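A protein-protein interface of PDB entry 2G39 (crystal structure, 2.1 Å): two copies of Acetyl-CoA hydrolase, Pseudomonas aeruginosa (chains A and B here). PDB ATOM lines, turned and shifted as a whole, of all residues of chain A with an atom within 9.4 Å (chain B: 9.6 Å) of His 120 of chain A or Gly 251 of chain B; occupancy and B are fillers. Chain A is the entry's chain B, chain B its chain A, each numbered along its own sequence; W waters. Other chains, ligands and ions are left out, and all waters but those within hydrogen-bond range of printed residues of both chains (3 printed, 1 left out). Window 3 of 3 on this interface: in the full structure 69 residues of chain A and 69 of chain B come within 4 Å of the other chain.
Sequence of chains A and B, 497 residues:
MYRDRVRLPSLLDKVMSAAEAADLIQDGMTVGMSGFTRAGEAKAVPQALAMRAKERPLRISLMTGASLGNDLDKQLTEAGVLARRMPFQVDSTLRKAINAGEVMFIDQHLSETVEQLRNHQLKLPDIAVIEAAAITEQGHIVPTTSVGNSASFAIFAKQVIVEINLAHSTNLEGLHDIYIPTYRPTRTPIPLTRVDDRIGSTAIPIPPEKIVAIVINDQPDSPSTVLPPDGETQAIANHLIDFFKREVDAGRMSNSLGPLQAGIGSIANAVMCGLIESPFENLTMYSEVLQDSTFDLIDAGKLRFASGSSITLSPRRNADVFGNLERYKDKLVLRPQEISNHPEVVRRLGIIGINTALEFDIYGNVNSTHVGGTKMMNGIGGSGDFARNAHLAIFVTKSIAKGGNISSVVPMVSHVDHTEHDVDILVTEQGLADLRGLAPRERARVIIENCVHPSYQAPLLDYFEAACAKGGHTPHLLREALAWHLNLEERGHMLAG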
ATOM      1  N   THR A 113      25.941 -15.584 -21.542  1.00  0.00           N
ATOM      2  CA  THR A 113      24.722 -15.017 -20.947  1.00  0.00           C
ATOM      3  C   THR A 113      25.047 -13.980 -19.838  1.00  0.00           C
ATOM      4  O   THR A 113      24.543 -12.871 -19.866  1.00  0.00           O
ATOM      5  CB  THR A 113      23.803 -16.140 -20.351  1.00  0.00           C
ATOM      6  OG1 THR A 113      23.609 -17.201 -21.312  1.00  0.00           O
ATOM      7  CG2 THR A 113      22.419 -15.576 -19.946  1.00  0.00           C
ATOM      8  N   VAL A 114      25.887 -14.343 -18.865  1.00  0.00           N
ATOM      9  CA  VAL A 114      26.180 -13.428 -17.764  1.00  0.00           C
ATOM     10  C   VAL A 114      26.974 -12.222 -18.236  1.00  0.00           C
ATOM     11  O   VAL A 114      26.834 -11.141 -17.668  1.00  0.00           O
ATOM     12  CB  VAL A 114      26.856 -14.116 -16.528  1.00  0.00           C
ATOM     13  CG1 VAL A 114      25.952 -15.236 -15.981  1.00  0.00           C
ATOM     14  CG2 VAL A 114      28.256 -14.646 -16.853  1.00  0.00           C
ATOM     15  N   GLU A 115      27.776 -12.382 -19.301  1.00  0.00           N
ATOM     16  CA  GLU A 115      28.491 -11.223 -19.853  1.00  0.00           C
ATOM     17  C   GLU A 115      27.481 -10.208 -20.436  1.00  0.00           C
ATOM     18  O   GLU A 115      27.616  -9.002 -20.254  1.00  0.00           O
ATOM     19  CB  GLU A 115      29.509 -11.676 -20.930  1.00  0.00           C
ATOM     20  CG  GLU A 115      30.482 -10.584 -21.367  1.00  0.00           C
ATOM     21  CD  GLU A 115      31.542 -10.285 -20.319  1.00  0.00           C
ATOM     22  OE1 GLU A 115      31.293  -9.444 -19.437  1.00  0.00           O
ATOM     23  OE2 GLU A 115      32.653 -10.868 -20.381  1.00  0.00           O
ATOM     24  N   GLN A 116      26.483 -10.710 -21.161  1.00  0.00           N
ATOM     25  CA  GLN A 116      25.405  -9.841 -21.700  1.00  0.00           C
ATOM     26  C   GLN A 116      24.659  -9.147 -20.564  1.00  0.00           C
ATOM     27  O   GLN A 116      24.453  -7.926 -20.597  1.00  0.00           O
ATOM     28  CB  GLN A 116      24.418 -10.663 -22.534  1.00  0.00           C
ATOM     29  CG  GLN A 116      25.026 -11.385 -23.686  1.00  0.00           C
ATOM     30  CD  GLN A 116      23.992 -12.191 -24.526  1.00  0.00           C
ATOM     31  OE1 GLN A 116      24.353 -12.808 -25.527  1.00  0.00           O
ATOM     32  NE2 GLN A 116      22.732 -12.155 -24.141  1.00  0.00           N
ATOM     33  N   LEU A 117      24.300  -9.927 -19.535  1.00  0.00           N
ATOM     34  CA  LEU A 117      23.575  -9.385 -18.395  1.00  0.00           C
ATOM     35  C   LEU A 117      24.330  -8.238 -17.749  1.00  0.00           C
ATOM     36  O   LEU A 117      23.764  -7.144 -17.525  1.00  0.00           O
ATOM     37  CB  LEU A 117      23.293 -10.478 -17.363  1.00  0.00           C
ATOM     38  CG  LEU A 117      22.228 -11.506 -17.768  1.00  0.00           C
ATOM     39  CD1 LEU A 117      22.253 -12.752 -16.871  1.00  0.00           C
ATOM     40  CD2 LEU A 117      20.827 -10.908 -17.790  1.00  0.00           C
ATOM     41  N   ARG A 118      25.612  -8.454 -17.483  1.00  0.00           N
ATOM     42  CA  ARG A 118      26.388  -7.454 -16.735  1.00  0.00           C
ATOM     43  C   ARG A 118      26.728  -6.179 -17.509  1.00  0.00           C
ATOM     44  O   ARG A 118      27.095  -5.155 -16.901  1.00  0.00           O
ATOM     45  CB  ARG A 118      27.631  -8.097 -16.080  1.00  0.00           C
ATOM     46  CG  ARG A 118      28.885  -8.191 -16.927  1.00  0.00           C
ATOM     47  CD  ARG A 118      30.137  -8.475 -16.098  1.00  0.00           C
ATOM     48  NE  ARG A 118      29.966  -9.758 -15.388  1.00  0.00           N
ATOM     49  CZ  ARG A 118      30.322 -10.944 -15.879  1.00  0.00           C
ATOM     50  NH1 ARG A 118      30.935 -11.041 -17.074  1.00  0.00           N
ATOM     51  NH2 ARG A 118      30.106 -12.043 -15.169  1.00  0.00           N
ATOM     52  N   ASN A 119      26.614  -6.233 -18.843  1.00  0.00           N
ATOM     53  CA  ASN A 119      26.941  -5.089 -19.715  1.00  0.00           C
ATOM     54  C   ASN A 119      25.727  -4.499 -20.447  1.00  0.00           C
ATOM     55  O   ASN A 119      25.871  -3.952 -21.510  1.00  0.00           O
ATOM     56  CB  ASN A 119      28.082  -5.446 -20.689  1.00  0.00           C
ATOM     57  CG  ASN A 119      29.349  -5.910 -19.946  1.00  0.00           C
ATOM     58  OD1 ASN A 119      30.062  -5.120 -19.312  1.00  0.00           O
ATOM     59  ND2 ASN A 119      29.614  -7.177 -20.020  1.00  0.00           N
ATOM     60  N   HIS A 120      24.550  -4.603 -19.819  1.00  0.00           N
ATOM     61  CA  HIS A 120      23.277  -3.991 -20.262  1.00  0.00           C
ATOM     62  C   HIS A 120      22.712  -4.532 -21.568  1.00  0.00           C
ATOM     63  O   HIS A 120      21.934  -3.839 -22.214  1.00  0.00           O
ATOM     64  CB  HIS A 120      23.407  -2.467 -20.400  1.00  0.00           C
ATOM     65  CG  HIS A 120      24.034  -1.810 -19.218  1.00  0.00           C
ATOM     66  ND1 HIS A 120      23.303  -1.374 -18.131  1.00  0.00           N
ATOM     67  CD2 HIS A 120      25.325  -1.487 -18.961  1.00  0.00           C
ATOM     68  CE1 HIS A 120      24.120  -0.823 -17.251  1.00  0.00           C
ATOM     69  NE2 HIS A 120      25.353  -0.892 -17.725  1.00  0.00           N
ATOM     70  N   GLN A 121      23.097  -5.749 -21.953  1.00  0.00           N
ATOM     71  CA  GLN A 121      22.697  -6.293 -23.240  1.00  0.00           C
ATOM     72  C   GLN A 121      21.522  -7.312 -23.190  1.00  0.00           C
ATOM     73  O   GLN A 121      21.067  -7.789 -24.240  1.00  0.00           O
ATOM     74  CB  GLN A 121      23.925  -6.914 -23.925  1.00  0.00           C
ATOM     75  CG  GLN A 121      25.112  -5.943 -24.109  1.00  0.00           C
ATOM     76  CD  GLN A 121      24.713  -4.665 -24.801  1.00  0.00           C
ATOM     77  OE1 GLN A 121      24.707  -3.583 -24.190  1.00  0.00           O
ATOM     78  NE2 GLN A 121      24.332  -4.771 -26.064  1.00  0.00           N
ATOM     79  N   LEU A 122      21.045  -7.626 -21.985  1.00  0.00           N
ATOM     80  CA  LEU A 122      20.010  -8.654 -21.756  1.00  0.00           C
ATOM     81  C   LEU A 122      19.324  -8.307 -20.435  1.00  0.00           C
ATOM     82  O   LEU A 122      19.990  -7.900 -19.474  1.00  0.00           O
ATOM     83  CB  LEU A 122      20.640 -10.035 -21.619  1.00  0.00           C
ATOM     84  CG  LEU A 122      19.830 -11.276 -21.946  1.00  0.00           C
ATOM     85  CD1 LEU A 122      19.381 -11.372 -23.440  1.00  0.00           C
ATOM     86  CD2 LEU A 122      20.606 -12.568 -21.499  1.00  0.00           C
ATOM     87  N   LYS A 123      18.001  -8.424 -20.406  1.00  0.00           N
ATOM     88  CA  LYS A 123      17.220  -8.068 -19.218  1.00  0.00           C
ATOM     89  C   LYS A 123      17.666  -8.854 -17.967  1.00  0.00           C
ATOM     90  O   LYS A 123      17.773 -10.094 -17.993  1.00  0.00           O
ATOM     91  CB  LYS A 123      15.740  -8.291 -19.465  1.00  0.00           C
ATOM     92  CG  LYS A 123      14.885  -7.958 -18.205  1.00  0.00           C
ATOM     93  CD  LYS A 123      13.459  -7.850 -18.581  1.00  0.00           C
ATOM     94  CE  LYS A 123      12.702  -7.191 -17.481  1.00  0.00           C
ATOM     95  NZ  LYS A 123      11.262  -7.562 -17.619  1.00  0.00           N
ATOM     96  N   LEU A 124      17.915  -8.126 -16.884  1.00  0.00           N
ATOM     97  CA  LEU A 124      18.292  -8.752 -15.619  1.00  0.00           C
ATOM     98  C   LEU A 124      17.187  -9.640 -15.013  1.00  0.00           C
ATOM     99  O   LEU A 124      15.995  -9.372 -15.220  1.00  0.00           O
ATOM    100  CB  LEU A 124      18.698  -7.677 -14.593  1.00  0.00           C
ATOM    101  CG  LEU A 124      19.977  -6.850 -14.843  1.00  0.00           C
ATOM    102  CD1 LEU A 124      20.206  -5.770 -13.717  1.00  0.00           C
ATOM    103  CD2 LEU A 124      21.214  -7.758 -15.034  1.00  0.00           C
ATOM    104  N   PHE A 156      22.765 -10.354  -9.533  1.00  0.00           N
ATOM    105  CA  PHE A 156      21.945  -9.450 -10.325  1.00  0.00           C
ATOM    106  C   PHE A 156      20.557  -9.220  -9.718  1.00  0.00           C
ATOM    107  O   PHE A 156      20.080  -8.100  -9.743  1.00  0.00           O
ATOM    108  CB  PHE A 156      21.741  -9.938 -11.761  1.00  0.00           C
ATOM    109  CG  PHE A 156      23.014 -10.036 -12.597  1.00  0.00           C
ATOM    110  CD1 PHE A 156      23.994  -9.021 -12.574  1.00  0.00           C
ATOM    111  CD2 PHE A 156      23.193 -11.111 -13.462  1.00  0.00           C
ATOM    112  CE1 PHE A 156      25.156  -9.110 -13.376  1.00  0.00           C
ATOM    113  CE2 PHE A 156      24.354 -11.205 -14.263  1.00  0.00           C
ATOM    114  CZ  PHE A 156      25.337 -10.203 -14.221  1.00  0.00           C
ATOM    115  N   TYR A 183      34.894  -5.533 -13.652  1.00  0.00           N
ATOM    116  CA  TYR A 183      34.051  -4.928 -14.642  1.00  0.00           C
ATOM    117  C   TYR A 183      34.788  -3.990 -15.569  1.00  0.00           C
ATOM    118  O   TYR A 183      35.748  -3.312 -15.172  1.00  0.00           O
ATOM    119  CB  TYR A 183      32.914  -4.169 -13.961  1.00  0.00           C
ATOM    120  CG  TYR A 183      31.879  -5.084 -13.286  1.00  0.00           C
ATOM    121  CD1 TYR A 183      31.926  -6.473 -13.430  1.00  0.00           C
ATOM    122  CD2 TYR A 183      30.836  -4.534 -12.549  1.00  0.00           C
ATOM    123  CE1 TYR A 183      30.968  -7.299 -12.817  1.00  0.00           C
ATOM    124  CE2 TYR A 183      29.858  -5.343 -11.961  1.00  0.00           C
ATOM    125  CZ  TYR A 183      29.932  -6.710 -12.093  1.00  0.00           C
ATOM    126  OH  TYR A 183      28.950  -7.467 -11.494  1.00  0.00           O
ATOM    127  N   ARG A 184      34.289  -3.923 -16.802  1.00  0.00           N
ATOM    128  CA  ARG A 184      34.729  -2.925 -17.755  1.00  0.00           C
ATOM    129  C   ARG A 184      34.355  -1.532 -17.236  1.00  0.00           C
ATOM    130  O   ARG A 184      33.425  -1.430 -16.453  1.00  0.00           O
ATOM    131  CB  ARG A 184      34.097  -3.200 -19.130  1.00  0.00           C
ATOM    132  CG  ARG A 184      34.220  -4.641 -19.587  1.00  0.00           C
ATOM    133  CD  ARG A 184      33.745  -4.786 -21.074  1.00  0.00           C
ATOM    134  NE  ARG A 184      33.736  -6.179 -21.549  1.00  0.00           N
ATOM    135  CZ  ARG A 184      32.720  -6.781 -22.174  1.00  0.00           C
ATOM    136  NH1 ARG A 184      31.583  -6.134 -22.435  1.00  0.00           N
ATOM    137  NH2 ARG A 184      32.857  -8.044 -22.570  1.00  0.00           N
ATOM    138  N   PHE B 243      20.799   4.267 -33.284  1.00  0.00           N
ATOM    139  CA  PHE B 243      20.815   3.149 -32.347  1.00  0.00           C
ATOM    140  C   PHE B 243      21.702   3.446 -31.123  1.00  0.00           C
ATOM    141  O   PHE B 243      21.250   3.299 -29.991  1.00  0.00           O
ATOM    142  CB  PHE B 243      21.209   1.842 -33.045  1.00  0.00           C
ATOM    143  CG  PHE B 243      21.568   0.744 -32.100  1.00  0.00           C
ATOM    144  CD1 PHE B 243      20.591  -0.112 -31.585  1.00  0.00           C
ATOM    145  CD2 PHE B 243      22.891   0.537 -31.735  1.00  0.00           C
ATOM    146  CE1 PHE B 243      20.948  -1.156 -30.688  1.00  0.00           C
ATOM    147  CE2 PHE B 243      23.243  -0.509 -30.852  1.00  0.00           C
ATOM    148  CZ  PHE B 243      22.275  -1.338 -30.336  1.00  0.00           C
ATOM    149  N   PHE B 244      22.947   3.854 -31.354  1.00  0.00           N
ATOM    150  CA  PHE B 244      23.837   4.225 -30.255  1.00  0.00           C
ATOM    151  C   PHE B 244      23.218   5.344 -29.402  1.00  0.00           C
ATOM    152  O   PHE B 244      23.354   5.311 -28.162  1.00  0.00           O
ATOM    153  CB  PHE B 244      25.187   4.724 -30.762  1.00  0.00           C
ATOM    154  CG  PHE B 244      26.072   3.674 -31.341  1.00  0.00           C
ATOM    155  CD1 PHE B 244      26.127   2.378 -30.800  1.00  0.00           C
ATOM    156  CD2 PHE B 244      26.905   3.990 -32.401  1.00  0.00           C
ATOM    157  CE1 PHE B 244      26.961   1.430 -31.337  1.00  0.00           C
ATOM    158  CE2 PHE B 244      27.754   3.038 -32.941  1.00  0.00           C
ATOM    159  CZ  PHE B 244      27.777   1.752 -32.412  1.00  0.00           C
ATOM    160  N   LYS B 245      22.547   6.323 -30.051  1.00  0.00           N
ATOM    161  CA  LYS B 245      21.870   7.415 -29.308  1.00  0.00           C
ATOM    162  C   LYS B 245      20.787   6.871 -28.380  1.00  0.00           C
ATOM    163  O   LYS B 245      20.677   7.306 -27.223  1.00  0.00           O
ATOM    164  CB  LYS B 245      21.295   8.530 -30.215  1.00  0.00           C
ATOM    165  CG  LYS B 245      22.323   9.453 -30.890  1.00  0.00           C
ATOM    166  CD  LYS B 245      21.591  10.641 -31.611  1.00  0.00           C
ATOM    167  CE  LYS B 245      22.544  11.546 -32.349  1.00  0.00           C
ATOM    168  NZ  LYS B 245      22.113  13.024 -32.490  1.00  0.00           N
ATOM    169  N   ARG B 246      20.002   5.908 -28.860  1.00  0.00           N
ATOM    170  CA  ARG B 246      18.977   5.289 -28.027  1.00  0.00           C
ATOM    171  C   ARG B 246      19.612   4.522 -26.865  1.00  0.00           C
ATOM    172  O   ARG B 246      19.061   4.513 -25.763  1.00  0.00           O
ATOM    173  CB  ARG B 246      18.124   4.308 -28.833  1.00  0.00           C
ATOM    174  CG  ARG B 246      17.137   4.935 -29.795  1.00  0.00           C
ATOM    175  CD  ARG B 246      16.151   3.879 -30.304  1.00  0.00           C
ATOM    176  NE  ARG B 246      16.777   2.776 -31.070  1.00  0.00           N
ATOM    177  CZ  ARG B 246      17.158   2.864 -32.348  1.00  0.00           C
ATOM    178  NH1 ARG B 246      17.691   1.811 -32.959  1.00  0.00           N
ATOM    179  NH2 ARG B 246      17.020   4.002 -33.021  1.00  0.00           N
ATOM    180  N   GLU B 247      20.744   3.866 -27.124  1.00  0.00           N
ATOM    181  CA  GLU B 247      21.476   3.116 -26.086  1.00  0.00           C
ATOM    182  C   GLU B 247      22.036   4.026 -24.989  1.00  0.00           C
ATOM    183  O   GLU B 247      21.929   3.704 -23.802  1.00  0.00           O
ATOM    184  CB  GLU B 247      22.627   2.289 -26.686  1.00  0.00           C
ATOM    185  CG  GLU B 247      22.175   1.116 -27.576  1.00  0.00           C
ATOM    186  CD  GLU B 247      21.228   0.184 -26.876  1.00  0.00           C
ATOM    187  OE1 GLU B 247      21.686  -0.614 -26.022  1.00  0.00           O
ATOM    188  OE2 GLU B 247      20.014   0.265 -27.160  1.00  0.00           O
ATOM    189  N   VAL B 248      22.671   5.126 -25.400  1.00  0.00           N
ATOM    190  CA  VAL B 248      23.191   6.126 -24.457  1.00  0.00           C
ATOM    191  C   VAL B 248      22.042   6.773 -23.660  1.00  0.00           C
ATOM    192  O   VAL B 248      22.026   6.759 -22.418  1.00  0.00           O
ATOM    193  CB  VAL B 248      24.050   7.210 -25.167  1.00  0.00           C
ATOM    194  CG1 VAL B 248      24.489   8.300 -24.178  1.00  0.00           C
ATOM    195  CG2 VAL B 248      25.256   6.601 -25.841  1.00  0.00           C
ATOM    196  N   ASP B 249      21.049   7.300 -24.362  1.00  0.00           N
ATOM    197  CA  ASP B 249      19.902   7.911 -23.668  1.00  0.00           C
ATOM    198  C   ASP B 249      19.196   6.913 -22.724  1.00  0.00           C
ATOM    199  O   ASP B 249      18.520   7.302 -21.781  1.00  0.00           O
ATOM    200  CB  ASP B 249      18.921   8.573 -24.665  1.00  0.00           C
ATOM    201  CG  ASP B 249      19.613   9.601 -25.644  1.00  0.00           C
ATOM    202  OD1 ASP B 249      20.782  10.046 -25.431  1.00  0.00           O
ATOM    203  OD2 ASP B 249      18.967   9.958 -26.667  1.00  0.00           O
ATOM    204  N   ALA B 250      19.368   5.616 -22.960  1.00  0.00           N
ATOM    205  CA  ALA B 250      18.750   4.589 -22.104  1.00  0.00           C
ATOM    206  C   ALA B 250      19.613   4.179 -20.893  1.00  0.00           C
ATOM    207  O   ALA B 250      19.209   3.346 -20.067  1.00  0.00           O
ATOM    208  CB  ALA B 250      18.350   3.364 -22.939  1.00  0.00           C
ATOM    209  N   GLY B 251      20.787   4.786 -20.785  1.00  0.00           N
ATOM    210  CA  GLY B 251      21.756   4.395 -19.779  1.00  0.00           C
ATOM    211  C   GLY B 251      22.396   3.035 -20.045  1.00  0.00           C
ATOM    212  O   GLY B 251      22.987   2.469 -19.143  1.00  0.00           O
ATOM    213  N   ARG B 252      22.290   2.506 -21.271  1.00  0.00           N
ATOM    214  CA  ARG B 252      22.913   1.225 -21.619  1.00  0.00           C
ATOM    215  C   ARG B 252      24.306   1.366 -22.260  1.00  0.00           C
ATOM    216  O   ARG B 252      24.988   0.372 -22.553  1.00  0.00           O
ATOM    217  CB  ARG B 252      21.989   0.404 -22.509  1.00  0.00           C
ATOM    218  CG  ARG B 252      20.679  -0.034 -21.825  1.00  0.00           C
ATOM    219  CD  ARG B 252      19.975  -1.128 -22.655  1.00  0.00           C
ATOM    220  NE  ARG B 252      19.556  -0.611 -23.959  1.00  0.00           N
ATOM    221  CZ  ARG B 252      18.371  -0.035 -24.194  1.00  0.00           C
ATOM    222  NH1 ARG B 252      17.470   0.088 -23.215  1.00  0.00           N
ATOM    223  NH2 ARG B 252      18.076   0.402 -25.408  1.00  0.00           N
ATOM    224  N   MET B 253      24.733   2.610 -22.456  1.00  0.00           N
ATOM    225  CA  MET B 253      26.032   2.901 -23.054  1.00  0.00           C
ATOM    226  C   MET B 253      26.406   4.327 -22.639  1.00  0.00           C
ATOM    227  O   MET B 253      25.528   5.133 -22.368  1.00  0.00           O
ATOM    228  CB  MET B 253      25.927   2.816 -24.581  1.00  0.00           C
ATOM    229  CG  MET B 253      27.246   2.874 -25.312  1.00  0.00           C
ATOM    230  SD  MET B 253      26.969   2.419 -27.201  1.00  0.00           S
ATOM    231  CE  MET B 253      26.932   0.428 -26.945  1.00  0.00           C
ATOM    232  N   SER B 254      27.694   4.633 -22.581  1.00  0.00           N
ATOM    233  CA  SER B 254      28.117   6.026 -22.357  1.00  0.00           C
ATOM    234  C   SER B 254      28.377   6.722 -23.690  1.00  0.00           C
ATOM    235  O   SER B 254      28.313   6.111 -24.771  1.00  0.00           O
ATOM    236  CB  SER B 254      29.362   6.116 -21.457  1.00  0.00           C
ATOM    237  OG  SER B 254      30.546   5.741 -22.155  1.00  0.00           O
ATOM    238  N   ASN B 255      28.693   8.006 -23.598  1.00  0.00           N
ATOM    239  CA  ASN B 255      28.857   8.820 -24.788  1.00  0.00           C
ATOM    240  C   ASN B 255      30.161   8.538 -25.565  1.00  0.00           C
ATOM    241  O   ASN B 255      30.311   8.917 -26.741  1.00  0.00           O
ATOM    242  CB  ASN B 255      28.722  10.294 -24.397  1.00  0.00           C
ATOM    243  CG  ASN B 255      28.330  11.151 -25.559  1.00  0.00           C
ATOM    244  OD1 ASN B 255      29.154  11.910 -26.061  1.00  0.00           O
ATOM    245  ND2 ASN B 255      27.077  11.019 -26.021  1.00  0.00           N
ATOM    246  N   HIS B 391      31.447  -6.920 -27.395  1.00  0.00           N
ATOM    247  CA  HIS B 391      30.328  -6.419 -26.585  1.00  0.00           C
ATOM    248  C   HIS B 391      29.122  -6.232 -27.492  1.00  0.00           C
ATOM    249  O   HIS B 391      27.988  -6.645 -27.146  1.00  0.00           O
ATOM    250  CB  HIS B 391      30.755  -5.119 -25.883  1.00  0.00           C
ATOM    251  CG  HIS B 391      29.633  -4.333 -25.270  1.00  0.00           C
ATOM    252  ND1 HIS B 391      28.802  -4.839 -24.279  1.00  0.00           N
ATOM    253  CD2 HIS B 391      29.276  -3.031 -25.435  1.00  0.00           C
ATOM    254  CE1 HIS B 391      27.954  -3.896 -23.902  1.00  0.00           C
ATOM    255  NE2 HIS B 391      28.215  -2.793 -24.592  1.00  0.00           N
ATOM    256  N   LEU B 392      29.370  -5.656 -28.674  1.00  0.00           N
ATOM    257  CA  LEU B 392      28.359  -5.617 -29.747  1.00  0.00           C
ATOM    258  C   LEU B 392      28.992  -6.006 -31.077  1.00  0.00           C
ATOM    259  O   LEU B 392      29.959  -5.368 -31.513  1.00  0.00           O
ATOM    260  CB  LEU B 392      27.753  -4.221 -29.923  1.00  0.00           C
ATOM    261  CG  LEU B 392      26.694  -3.697 -28.958  1.00  0.00           C
ATOM    262  CD1 LEU B 392      26.775  -2.203 -28.918  1.00  0.00           C
ATOM    263  CD2 LEU B 392      25.293  -4.123 -29.423  1.00  0.00           C
ATOM    264  N   ASP B 434      17.882  -4.993 -34.344  1.00  0.00           N
ATOM    265  CA  ASP B 434      18.458  -5.221 -33.063  1.00  0.00           C
ATOM    266  C   ASP B 434      18.025  -6.618 -32.685  1.00  0.00           C
ATOM    267  O   ASP B 434      16.851  -6.867 -32.487  1.00  0.00           O
ATOM    268  CB  ASP B 434      17.891  -4.202 -32.042  1.00  0.00           C
ATOM    269  CG  ASP B 434      18.451  -4.405 -30.642  1.00  0.00           C
ATOM    270  OD1 ASP B 434      19.129  -5.435 -30.416  1.00  0.00           O
ATOM    271  OD2 ASP B 434      18.222  -3.539 -29.757  1.00  0.00           O
ATOM    272  N   ARG B 436      19.263  -8.543 -30.113  1.00  0.00           N
ATOM    273  CA  ARG B 436      19.626  -8.930 -28.735  1.00  0.00           C
ATOM    274  C   ARG B 436      18.442  -9.581 -27.999  1.00  0.00           C
ATOM    275  O   ARG B 436      17.341  -9.056 -27.988  1.00  0.00           O
ATOM    276  CB  ARG B 436      20.209  -7.710 -27.963  1.00  0.00           C
ATOM    277  CG  ARG B 436      21.533  -7.205 -28.567  1.00  0.00           C
ATOM    278  CD  ARG B 436      21.995  -5.901 -27.957  1.00  0.00           C
ATOM    279  NE  ARG B 436      20.971  -4.872 -28.144  1.00  0.00           N
ATOM    280  CZ  ARG B 436      20.949  -3.686 -27.527  1.00  0.00           C
ATOM    281  NH1 ARG B 436      21.918  -3.318 -26.674  1.00  0.00           N
ATOM    282  NH2 ARG B 436      19.947  -2.865 -27.767  1.00  0.00           N
ATOM    283  N   GLY B 437      18.687 -10.758 -27.434  1.00  0.00           N
ATOM    284  CA  GLY B 437      17.682 -11.466 -26.645  1.00  0.00           C
ATOM    285  C   GLY B 437      16.524 -12.044 -27.435  1.00  0.00           C
ATOM    286  O   GLY B 437      15.557 -12.484 -26.828  1.00  0.00           O
HETATM  287  O   HOH W   1      18.259  -8.025 -25.003  1.00  0.00           O
HETATM  288  O   HOH W   2      30.890  -3.299 -22.287  1.00  0.00           O
HETATM  289  O   HOH W   3      25.321  -6.767 -27.383  1.00  0.00           O
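The side-chain amide nitrogen (NE2) of Gln 121 of chain A sits close to the guanidinium group (NH1) of Arg 436 of chain B (2.9 Å).
The guanidinium group of Arg 252 of chain B is in salt-bridge range of the side-chain carboxylate of Glu 247 of chain B (2.6 Å).
OD2 of Asp 434 of chain B lies within salt-bridge range of NH2 of Arg 436 of chain B (2.7 Å).
The side-chain carboxylate (OE2) of Glu 115 of chain A is in salt-bridge range of the guanidinium group (NH2) of Arg 184 of chain A (3.6 Å).
The backbone carbonyl oxygen (O) of Gln 116 of chain A sits at hydrogen-bond distance from the backbone NH (N) of Gln 121 of chain A (2.9 Å).
The side-chain amide nitrogen (ND2) of Asn 119 of chain A lies within hydrogen-bond range of the backbone carbonyl oxygen (O) of Glu 115 of chain A (2.7 Å).
The side-chain amide nitrogen (ND2) of Asn 119 of chain A lies close to the guanidinium group (NH1) of Arg 184 of chain A.
Among the printed residues, merely in contact across the chains: Asn 119 of chain A with His 391 of chain B, His 120 of chain A with Gly 251 of chain B, His 120 of chain A with Arg 252 of chain B, Gln 121 of chain A with His 391 of chain B, Gln 121 of chain A with Leu 392 of chain B, Leu 122 of chain A with Gly 437 of chain B and Arg 184 of chain A with His 391 of chain B.
Of the printed residues of chain B, His 120 of chain A touches Gly 251 and Arg 252.
Of chain B, only His 391, Leu 392 and Arg 436 come within 4 Å of Gln 121 of chain A.
Of the printed residues of chain B, Arg 184 of chain A touches His 391.
No residue of chain A comes within 4 Å of Ala 250 of chain B.
Gly 251 of chain B touches one residue of chain A.
Printed residues of chain A within 4 Å of Arg 436 of chain B: Gln 121 (2.9 Å).
The nearest residue of chain B that does not touch His 120 of chain A is Arg 436 of chain B (4.5 Å).
The nearest residue of chain A that does not touch Gly 251 of chain B is Asn 119 of chain A (7.4 Å).
The nearest printed residue of chain A that does not touch Arg 252 of chain B is Gln 121 of chain A (4.3 Å).
Of the 15 printed residues of chain A, 5 touch a printed residue of chain B.
Of the 18 printed residues of chain B, 6 touch a printed residue of chain A.
Hydrophobic or aromatic side chains of chain B that line the printed part of chain A: His 391 and Leu 392.
No position is printed for both chains.
Of the 8 pairs that touch across the chains among the printed residues, none has its exchanged pair printed and touching as well.
Water W3 lies within hydrogen-bond range of the side-chain amide nitrogen of Gln 121 of chain A (2.6 Å) and the backbone carbonyl oxygen of His 391 of chain B (2.7 Å).
Water W1 bridges O of Gln 121 of chain A and O of Arg 436 of chain B.
Water W2 lies within hydrogen-bond range of NH1 of Arg 184 of chain A (2.9 Å) and ND1 of His 391 of chain B (3.3 Å).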
